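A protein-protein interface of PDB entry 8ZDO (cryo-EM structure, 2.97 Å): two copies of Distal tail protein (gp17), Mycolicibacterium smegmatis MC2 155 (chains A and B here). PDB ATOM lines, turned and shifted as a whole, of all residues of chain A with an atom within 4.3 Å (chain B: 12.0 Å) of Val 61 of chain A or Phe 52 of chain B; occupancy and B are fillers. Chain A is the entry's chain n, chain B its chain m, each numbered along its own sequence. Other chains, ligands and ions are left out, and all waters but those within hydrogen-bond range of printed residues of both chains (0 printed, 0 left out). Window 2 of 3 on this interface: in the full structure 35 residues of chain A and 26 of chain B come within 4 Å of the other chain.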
ATOM      1  N   PRO A  42      15.386  12.017 -13.008  1.00  0.00           N
ATOM      2  CA  PRO A  42      15.546  12.713 -11.724  1.00  0.00           C
ATOM      3  C   PRO A  42      15.048  11.848 -10.578  1.00  0.00           C
ATOM      4  O   PRO A  42      13.871  11.490 -10.519  1.00  0.00           O
ATOM      5  CB  PRO A  42      14.695  13.976 -11.896  1.00  0.00           C
ATOM      6  CG  PRO A  42      13.709  13.620 -12.947  1.00  0.00           C
ATOM      7  CD  PRO A  42      14.412  12.687 -13.882  1.00  0.00           C
ATOM      8  N   VAL A  43      15.955  11.507  -9.669  1.00  0.00           N
ATOM      9  CA  VAL A  43      15.640  10.726  -8.482  1.00  0.00           C
ATOM     10  C   VAL A  43      16.074  11.528  -7.266  1.00  0.00           C
ATOM     11  O   VAL A  43      17.189  12.058  -7.235  1.00  0.00           O
ATOM     12  CB  VAL A  43      16.331   9.352  -8.501  1.00  0.00           C
ATOM     13  CG1 VAL A  43      15.888   8.524  -7.314  1.00  0.00           C
ATOM     14  CG2 VAL A  43      16.032   8.627  -9.795  1.00  0.00           C
ATOM     15  N   ARG A  60      12.968   8.309  -4.249  1.00  0.00           N
ATOM     16  CA  ARG A  60      11.755   8.552  -5.014  1.00  0.00           C
ATOM     17  C   ARG A  60      12.148   9.154  -6.351  1.00  0.00           C
ATOM     18  O   ARG A  60      12.935  10.103  -6.398  1.00  0.00           O
ATOM     19  CB  ARG A  60      10.799   9.493  -4.274  1.00  0.00           C
ATOM     20  CG  ARG A  60      10.377   9.012  -2.900  1.00  0.00           C
ATOM     21  CD  ARG A  60       9.222   8.034  -2.988  1.00  0.00           C
ATOM     22  NE  ARG A  60       8.680   7.697  -1.678  1.00  0.00           N
ATOM     23  CZ  ARG A  60       9.259   6.873  -0.814  1.00  0.00           C
ATOM     24  NH1 ARG A  60      10.408   6.280  -1.089  1.00  0.00           N
ATOM     25  NH2 ARG A  60       8.667   6.638   0.352  1.00  0.00           N
ATOM     26  N   VAL A  61      11.613   8.606  -7.425  1.00  0.00           N
ATOM     27  CA  VAL A  61      11.864   9.131  -8.760  1.00  0.00           C
ATOM     28  C   VAL A  61      10.876  10.255  -9.034  1.00  0.00           C
ATOM     29  O   VAL A  61       9.712  10.194  -8.626  1.00  0.00           O
ATOM     30  CB  VAL A  61      11.774   8.015  -9.819  1.00  0.00           C
ATOM     31  CG1 VAL A  61      10.367   7.451  -9.904  1.00  0.00           C
ATOM     32  CG2 VAL A  61      12.238   8.527 -11.171  1.00  0.00           C
ATOM     33  N   GLN A  62      11.350  11.301  -9.700  1.00  0.00           N
ATOM     34  CA  GLN A  62      10.558  12.488  -9.978  1.00  0.00           C
ATOM     35  C   GLN A  62      10.237  12.563 -11.463  1.00  0.00           C
ATOM     36  O   GLN A  62      10.959  12.014 -12.298  1.00  0.00           O
ATOM     37  CB  GLN A  62      11.302  13.750  -9.540  1.00  0.00           C
ATOM     38  CG  GLN A  62      11.911  13.655  -8.153  1.00  0.00           C
ATOM     39  CD  GLN A  62      10.868  13.672  -7.059  1.00  0.00           C
ATOM     40  OE1 GLN A  62      10.566  12.644  -6.457  1.00  0.00           O
ATOM     41  NE2 GLN A  62      10.310  14.844  -6.794  1.00  0.00           N
ATOM     42  N   THR A 141       5.681  12.594 -17.519  1.00  0.00           N
ATOM     43  CA  THR A 141       5.019  12.024 -16.352  1.00  0.00           C
ATOM     44  C   THR A 141       5.634  10.684 -15.974  1.00  0.00           C
ATOM     45  O   THR A 141       5.865  10.408 -14.791  1.00  0.00           O
ATOM     46  CB  THR A 141       3.524  11.879 -16.633  1.00  0.00           C
ATOM     47  OG1 THR A 141       2.926  13.178 -16.719  1.00  0.00           O
ATOM     48  CG2 THR A 141       2.837  11.070 -15.551  1.00  0.00           C
ATOM     49  N   PHE A 142       5.906   9.837 -16.966  1.00  0.00           N
ATOM     50  CA  PHE A 142       6.676   8.624 -16.746  1.00  0.00           C
ATOM     51  C   PHE A 142       8.126   8.928 -17.084  1.00  0.00           C
ATOM     52  O   PHE A 142       8.484   8.982 -18.269  1.00  0.00           O
ATOM     53  CB  PHE A 142       6.150   7.477 -17.607  1.00  0.00           C
ATOM     54  CG  PHE A 142       6.653   6.138 -17.183  1.00  0.00           C
ATOM     55  CD1 PHE A 142       6.261   5.596 -15.977  1.00  0.00           C
ATOM     56  CD2 PHE A 142       7.526   5.424 -17.979  1.00  0.00           C
ATOM     57  CE1 PHE A 142       6.722   4.371 -15.576  1.00  0.00           C
ATOM     58  CE2 PHE A 142       7.989   4.197 -17.582  1.00  0.00           C
ATOM     59  CZ  PHE A 142       7.588   3.672 -16.377  1.00  0.00           C
ATOM     60  N   PRO A 143       8.999   9.123 -16.095  1.00  0.00           N
ATOM     61  CA  PRO A 143      10.330   9.675 -16.367  1.00  0.00           C
ATOM     62  C   PRO A 143      11.306   8.705 -17.010  1.00  0.00           C
ATOM     63  O   PRO A 143      12.417   9.120 -17.356  1.00  0.00           O
ATOM     64  CB  PRO A 143      10.813  10.085 -14.971  1.00  0.00           C
ATOM     65  CG  PRO A 143      10.128   9.146 -14.057  1.00  0.00           C
ATOM     66  CD  PRO A 143       8.801   8.817 -14.669  1.00  0.00           C
ATOM     67  N   TYR A 144      10.935   7.442 -17.186  1.00  0.00           N
ATOM     68  CA  TYR A 144      11.852   6.442 -17.706  1.00  0.00           C
ATOM     69  C   TYR A 144      11.803   6.401 -19.226  1.00  0.00           C
ATOM     70  O   TYR A 144      10.725   6.423 -19.825  1.00  0.00           O
ATOM     71  CB  TYR A 144      11.517   5.062 -17.145  1.00  0.00           C
ATOM     72  CG  TYR A 144      11.737   4.943 -15.660  1.00  0.00           C
ATOM     73  CD1 TYR A 144      12.944   5.309 -15.089  1.00  0.00           C
ATOM     74  CD2 TYR A 144      10.737   4.468 -14.828  1.00  0.00           C
ATOM     75  CE1 TYR A 144      13.150   5.205 -13.736  1.00  0.00           C
ATOM     76  CE2 TYR A 144      10.933   4.362 -13.473  1.00  0.00           C
ATOM     77  CZ  TYR A 144      12.142   4.731 -12.931  1.00  0.00           C
ATOM     78  OH  TYR A 144      12.345   4.623 -11.576  1.00  0.00           O
ATOM     79  N   TRP A 176       6.971  -3.653 -14.360  1.00  0.00           N
ATOM     80  CA  TRP A 176       5.751  -4.305 -13.906  1.00  0.00           C
ATOM     81  C   TRP A 176       5.102  -5.036 -15.071  1.00  0.00           C
ATOM     82  O   TRP A 176       4.888  -4.450 -16.135  1.00  0.00           O
ATOM     83  CB  TRP A 176       4.780  -3.290 -13.308  1.00  0.00           C
ATOM     84  CG  TRP A 176       5.350  -2.533 -12.158  1.00  0.00           C
ATOM     85  CD1 TRP A 176       6.085  -1.389 -12.217  1.00  0.00           C
ATOM     86  CD2 TRP A 176       5.240  -2.868 -10.772  1.00  0.00           C
ATOM     87  NE1 TRP A 176       6.437  -0.989 -10.953  1.00  0.00           N
ATOM     88  CE2 TRP A 176       5.929  -1.881 -10.049  1.00  0.00           C
ATOM     89  CE3 TRP A 176       4.623  -3.908 -10.074  1.00  0.00           C
ATOM     90  CZ2 TRP A 176       6.018  -1.901  -8.662  1.00  0.00           C
ATOM     91  CZ3 TRP A 176       4.711  -3.924  -8.700  1.00  0.00           C
ATOM     92  CH2 TRP A 176       5.404  -2.928  -8.008  1.00  0.00           C
ATOM     93  N   ASP A 226       1.143  -3.037 -12.528  1.00  0.00           N
ATOM     94  CA  ASP A 226       1.531  -1.642 -12.390  1.00  0.00           C
ATOM     95  C   ASP A 226       0.719  -0.978 -11.284  1.00  0.00           C
ATOM     96  O   ASP A 226      -0.514  -1.097 -11.269  1.00  0.00           O
ATOM     97  CB  ASP A 226       1.313  -0.905 -13.711  1.00  0.00           C
ATOM     98  CG  ASP A 226       2.334   0.185 -13.951  1.00  0.00           C
ATOM     99  OD1 ASP A 226       3.294   0.294 -13.164  1.00  0.00           O
ATOM    100  OD2 ASP A 226       2.177   0.938 -14.933  1.00  0.00           O
ATOM    101  N   PRO A 227       1.361  -0.291 -10.337  1.00  0.00           N
ATOM    102  CA  PRO A 227       0.599   0.394  -9.281  1.00  0.00           C
ATOM    103  C   PRO A 227      -0.308   1.496  -9.795  1.00  0.00           C
ATOM    104  O   PRO A 227      -1.249   1.878  -9.091  1.00  0.00           O
ATOM    105  CB  PRO A 227       1.693   0.954  -8.364  1.00  0.00           C
ATOM    106  CG  PRO A 227       2.926   0.974  -9.202  1.00  0.00           C
ATOM    107  CD  PRO A 227       2.812  -0.190 -10.120  1.00  0.00           C
ATOM    108  N   ARG A 228      -0.052   2.025 -10.993  1.00  0.00           N
ATOM    109  CA  ARG A 228      -0.882   3.107 -11.515  1.00  0.00           C
ATOM    110  C   ARG A 228      -2.313   2.643 -11.756  1.00  0.00           C
ATOM    111  O   ARG A 228      -3.264   3.390 -11.503  1.00  0.00           O
ATOM    112  CB  ARG A 228      -0.280   3.659 -12.807  1.00  0.00           C
ATOM    113  CG  ARG A 228       1.233   3.762 -12.803  1.00  0.00           C
ATOM    114  CD  ARG A 228       1.710   4.957 -13.611  1.00  0.00           C
ATOM    115  NE  ARG A 228       1.610   4.738 -15.049  1.00  0.00           N
ATOM    116  CZ  ARG A 228       2.500   4.072 -15.771  1.00  0.00           C
ATOM    117  NH1 ARG A 228       3.565   3.519 -15.217  1.00  0.00           N
ATOM    118  NH2 ARG A 228       2.316   3.956 -17.083  1.00  0.00           N
ATOM    119  N   TRP A 281      12.062  -0.461 -19.540  1.00  0.00           N
ATOM    120  CA  TRP A 281      12.270   0.886 -19.033  1.00  0.00           C
ATOM    121  C   TRP A 281      13.745   1.129 -18.750  1.00  0.00           C
ATOM    122  O   TRP A 281      14.431   0.274 -18.184  1.00  0.00           O
ATOM    123  CB  TRP A 281      11.455   1.120 -17.763  1.00  0.00           C
ATOM    124  CG  TRP A 281       9.987   0.999 -17.971  1.00  0.00           C
ATOM    125  CD1 TRP A 281       9.310   1.174 -19.137  1.00  0.00           C
ATOM    126  CD2 TRP A 281       9.006   0.676 -16.982  1.00  0.00           C
ATOM    127  NE1 TRP A 281       7.969   0.981 -18.939  1.00  0.00           N
ATOM    128  CE2 TRP A 281       7.756   0.671 -17.623  1.00  0.00           C
ATOM    129  CE3 TRP A 281       9.063   0.389 -15.617  1.00  0.00           C
ATOM    130  CZ2 TRP A 281       6.575   0.391 -16.949  1.00  0.00           C
ATOM    131  CZ3 TRP A 281       7.892   0.112 -14.951  1.00  0.00           C
ATOM    132  CH2 TRP A 281       6.665   0.115 -15.614  1.00  0.00           C
ATOM    133  N   TYR B  47      -0.543  18.485 -11.603  1.00  0.00           N
ATOM    134  CA  TYR B  47       0.035  17.172 -11.355  1.00  0.00           C
ATOM    135  C   TYR B  47      -0.253  16.727  -9.932  1.00  0.00           C
ATOM    136  O   TYR B  47      -0.142  17.517  -8.992  1.00  0.00           O
ATOM    137  CB  TYR B  47       1.545  17.177 -11.610  1.00  0.00           C
ATOM    138  CG  TYR B  47       1.911  17.719 -12.967  1.00  0.00           C
ATOM    139  CD1 TYR B  47       1.824  16.925 -14.100  1.00  0.00           C
ATOM    140  CD2 TYR B  47       2.326  19.031 -13.118  1.00  0.00           C
ATOM    141  CE1 TYR B  47       2.148  17.420 -15.343  1.00  0.00           C
ATOM    142  CE2 TYR B  47       2.652  19.534 -14.355  1.00  0.00           C
ATOM    143  CZ  TYR B  47       2.562  18.724 -15.464  1.00  0.00           C
ATOM    144  OH  TYR B  47       2.887  19.226 -16.700  1.00  0.00           O
ATOM    145  N   VAL B  48      -0.625  15.460  -9.783  1.00  0.00           N
ATOM    146  CA  VAL B  48      -0.860  14.848  -8.478  1.00  0.00           C
ATOM    147  C   VAL B  48       0.310  13.924  -8.168  1.00  0.00           C
ATOM    148  O   VAL B  48       0.964  13.431  -9.096  1.00  0.00           O
ATOM    149  CB  VAL B  48      -2.192  14.080  -8.447  1.00  0.00           C
ATOM    150  CG1 VAL B  48      -3.313  14.944  -8.968  1.00  0.00           C
ATOM    151  CG2 VAL B  48      -2.094  12.805  -9.263  1.00  0.00           C
ATOM    152  N   PRO B  49       0.628  13.678  -6.899  1.00  0.00           N
ATOM    153  CA  PRO B  49       1.672  12.697  -6.584  1.00  0.00           C
ATOM    154  C   PRO B  49       1.282  11.304  -7.056  1.00  0.00           C
ATOM    155  O   PRO B  49       0.113  10.917  -7.013  1.00  0.00           O
ATOM    156  CB  PRO B  49       1.779  12.766  -5.057  1.00  0.00           C
ATOM    157  CG  PRO B  49       1.193  14.075  -4.688  1.00  0.00           C
ATOM    158  CD  PRO B  49       0.126  14.352  -5.692  1.00  0.00           C
ATOM    159  N   GLY B  50       2.278  10.546  -7.502  1.00  0.00           N
ATOM    160  CA  GLY B  50       2.053   9.204  -7.979  1.00  0.00           C
ATOM    161  C   GLY B  50       3.224   8.288  -7.696  1.00  0.00           C
ATOM    162  O   GLY B  50       4.271   8.714  -7.201  1.00  0.00           O
ATOM    163  N   PRO B  51       3.063   6.999  -8.002  1.00  0.00           N
ATOM    164  CA  PRO B  51       4.155   6.044  -7.754  1.00  0.00           C
ATOM    165  C   PRO B  51       5.428   6.358  -8.517  1.00  0.00           C
ATOM    166  O   PRO B  51       6.523   6.090  -8.010  1.00  0.00           O
ATOM    167  CB  PRO B  51       3.550   4.704  -8.192  1.00  0.00           C
ATOM    168  CG  PRO B  51       2.445   5.070  -9.120  1.00  0.00           C
ATOM    169  CD  PRO B  51       1.884   6.348  -8.592  1.00  0.00           C
ATOM    170  N   PHE B  52       5.320   6.911  -9.724  1.00  0.00           N
ATOM    171  CA  PHE B  52       6.474   7.225 -10.555  1.00  0.00           C
ATOM    172  C   PHE B  52       6.759   8.722 -10.581  1.00  0.00           C
ATOM    173  O   PHE B  52       7.199   9.259 -11.599  1.00  0.00           O
ATOM    174  CB  PHE B  52       6.271   6.694 -11.972  1.00  0.00           C
ATOM    175  CG  PHE B  52       6.150   5.202 -12.044  1.00  0.00           C
ATOM    176  CD1 PHE B  52       7.276   4.403 -11.993  1.00  0.00           C
ATOM    177  CD2 PHE B  52       4.913   4.597 -12.157  1.00  0.00           C
ATOM    178  CE1 PHE B  52       7.170   3.033 -12.057  1.00  0.00           C
ATOM    179  CE2 PHE B  52       4.803   3.226 -12.221  1.00  0.00           C
ATOM    180  CZ  PHE B  52       5.932   2.443 -12.171  1.00  0.00           C
ATOM    181  N   GLY B  53       6.523   9.401  -9.466  1.00  0.00           N
ATOM    182  CA  GLY B  53       6.683  10.838  -9.413  1.00  0.00           C
ATOM    183  C   GLY B  53       5.353  11.552  -9.327  1.00  0.00           C
ATOM    184  O   GLY B  53       4.690  11.516  -8.288  1.00  0.00           O
ATOM    185  N   GLU B  54       4.950  12.200 -10.414  1.00  0.00           N
ATOM    186  CA  GLU B  54       3.692  12.924 -10.461  1.00  0.00           C
ATOM    187  C   GLU B  54       2.904  12.498 -11.689  1.00  0.00           C
ATOM    188  O   GLU B  54       3.479  12.156 -12.724  1.00  0.00           O
ATOM    189  CB  GLU B  54       3.916  14.439 -10.477  1.00  0.00           C
ATOM    190  CG  GLU B  54       4.092  15.038  -9.096  1.00  0.00           C
ATOM    191  CD  GLU B  54       4.283  16.539  -9.129  1.00  0.00           C
ATOM    192  OE1 GLU B  54       5.157  17.011  -9.883  1.00  0.00           O
ATOM    193  OE2 GLU B  54       3.562  17.246  -8.396  1.00  0.00           O
ATOM    194  N   GLU B  55       1.581  12.520 -11.562  1.00  0.00           N
ATOM    195  CA  GLU B  55       0.671  12.132 -12.630  1.00  0.00           C
ATOM    196  C   GLU B  55      -0.079  13.356 -13.137  1.00  0.00           C
ATOM    197  O   GLU B  55      -0.406  14.257 -12.361  1.00  0.00           O
ATOM    198  CB  GLU B  55      -0.330  11.080 -12.146  1.00  0.00           C
ATOM    199  CG  GLU B  55       0.300   9.787 -11.657  1.00  0.00           C
ATOM    200  CD  GLU B  55       0.940   8.982 -12.770  1.00  0.00           C
ATOM    201  OE1 GLU B  55       0.408   9.000 -13.901  1.00  0.00           O
ATOM    202  OE2 GLU B  55       1.974   8.330 -12.515  1.00  0.00           O
ATOM    203  N   TYR B  56      -0.351  13.381 -14.438  1.00  0.00           N
ATOM    204  CA  TYR B  56      -1.073  14.498 -15.037  1.00  0.00           C
ATOM    205  C   TYR B  56      -2.477  14.603 -14.456  1.00  0.00           C
ATOM    206  O   TYR B  56      -3.194  13.605 -14.347  1.00  0.00           O
ATOM    207  CB  TYR B  56      -1.137  14.319 -16.552  1.00  0.00           C
ATOM    208  CG  TYR B  56      -1.724  15.493 -17.298  1.00  0.00           C
ATOM    209  CD1 TYR B  56      -1.066  16.713 -17.342  1.00  0.00           C
ATOM    210  CD2 TYR B  56      -2.931  15.377 -17.971  1.00  0.00           C
ATOM    211  CE1 TYR B  56      -1.598  17.781 -18.028  1.00  0.00           C
ATOM    212  CE2 TYR B  56      -3.468  16.441 -18.658  1.00  0.00           C
ATOM    213  CZ  TYR B  56      -2.798  17.638 -18.684  1.00  0.00           C
ATOM    214  OH  TYR B  56      -3.335  18.700 -19.371  1.00  0.00           O
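The backbone NH (N) of Gly 53 of chain B lies close to the backbone carbonyl oxygen (O) of Val 61 of chain A, 3.4 Å away.
OD2 of Asp 226 of chain A lies within salt-bridge range of NH1 of Arg 228 of chain A (2.9 Å). The backbone carbonyl oxygen (O) of Val 48 of chain B is in hydrogen-bond range of the backbone NH (N) of Glu 55 of chain B (2.7 Å).
Among the printed residues, pairs that only touch across the chains: Val 61 of chain A with Phe 52 of chain B, Thr 141 of chain A with Phe 52 of chain B, Thr 141 of chain A with Glu 54 of chain B, Thr 141 of chain A with Glu 55 of chain B, Thr 141 of chain A with Tyr 56 of chain B, Phe 142 of chain A with Phe 52 of chain B, Pro 143 of chain A with Phe 52 of chain B, Tyr 144 of chain A with Phe 52 of chain B, Trp 176 of chain A with Phe 52 of chain B, Asp 226 of chain A with Phe 52 of chain B, Pro 227 of chain A with Pro 51 of chain B, Arg 228 of chain A with Phe 52 of chain B and Arg 228 of chain A with Glu 55 of chain B.
No residue of chain B comes within 4 Å of Pro 42 of chain A. Val 61 of chain A touches just these residues of chain B: Phe 52 and Gly 53. Of chain B, only Phe 52 comes within 4 Å of Pro 143 of chain A. Of the printed residues of chain B, Tyr 144 of chain A touches Phe 52. Of the printed residues of chain B, Trp 176 of chain A touches Phe 52 (3.7 Å). Asp 226 of chain A touches just one residue of chain B: Phe 52 (3.4 Å). Pro 49 of chain B touches none of the printed residues of chain A. Printed residues of chain A within 4 Å of Pro 51 of chain B: Pro 227. Of chain A, only Val 61, Thr 141, Phe 142, Pro 143, Tyr 144, Trp 176, Asp 226 and Arg 228 come within 4 Å of Phe 52 of chain B. Of the printed residues of chain A, Tyr 56 of chain B touches Thr 141. The nearest residue of chain B that does not touch Val 61 of chain A is Pro 51 of chain B (4.5 Å). The nearest residue of chain A that does not touch Phe 52 of chain B is Trp 281 of chain A (4.1 Å). The nearest printed residue of chain A that does not touch Pro 51 of chain B is Arg 228 of chain A (4.1 Å).
Of the 10 printed residues of chain B, 6 touch a printed residue of chain A. Hydrophobic or aromatic side chains of chain B that line the printed part of chain A: Pro 51 and Phe 52. Printed residues of chain A that touch a printed residue of chain B: Val 61, Thr 141, Phe 142, Pro 143, Tyr 144, Trp 176, Asp 226, Pro 227 and Arg 228. Along chain A the printed residues that touch a printed residue of chain B span positions 61 to 228. Among the printed residues, no Asp or Glu carboxylate lies within 4 Å of a Lys or Arg side-chain nitrogen of the other chain.
No position is printed for both chains.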
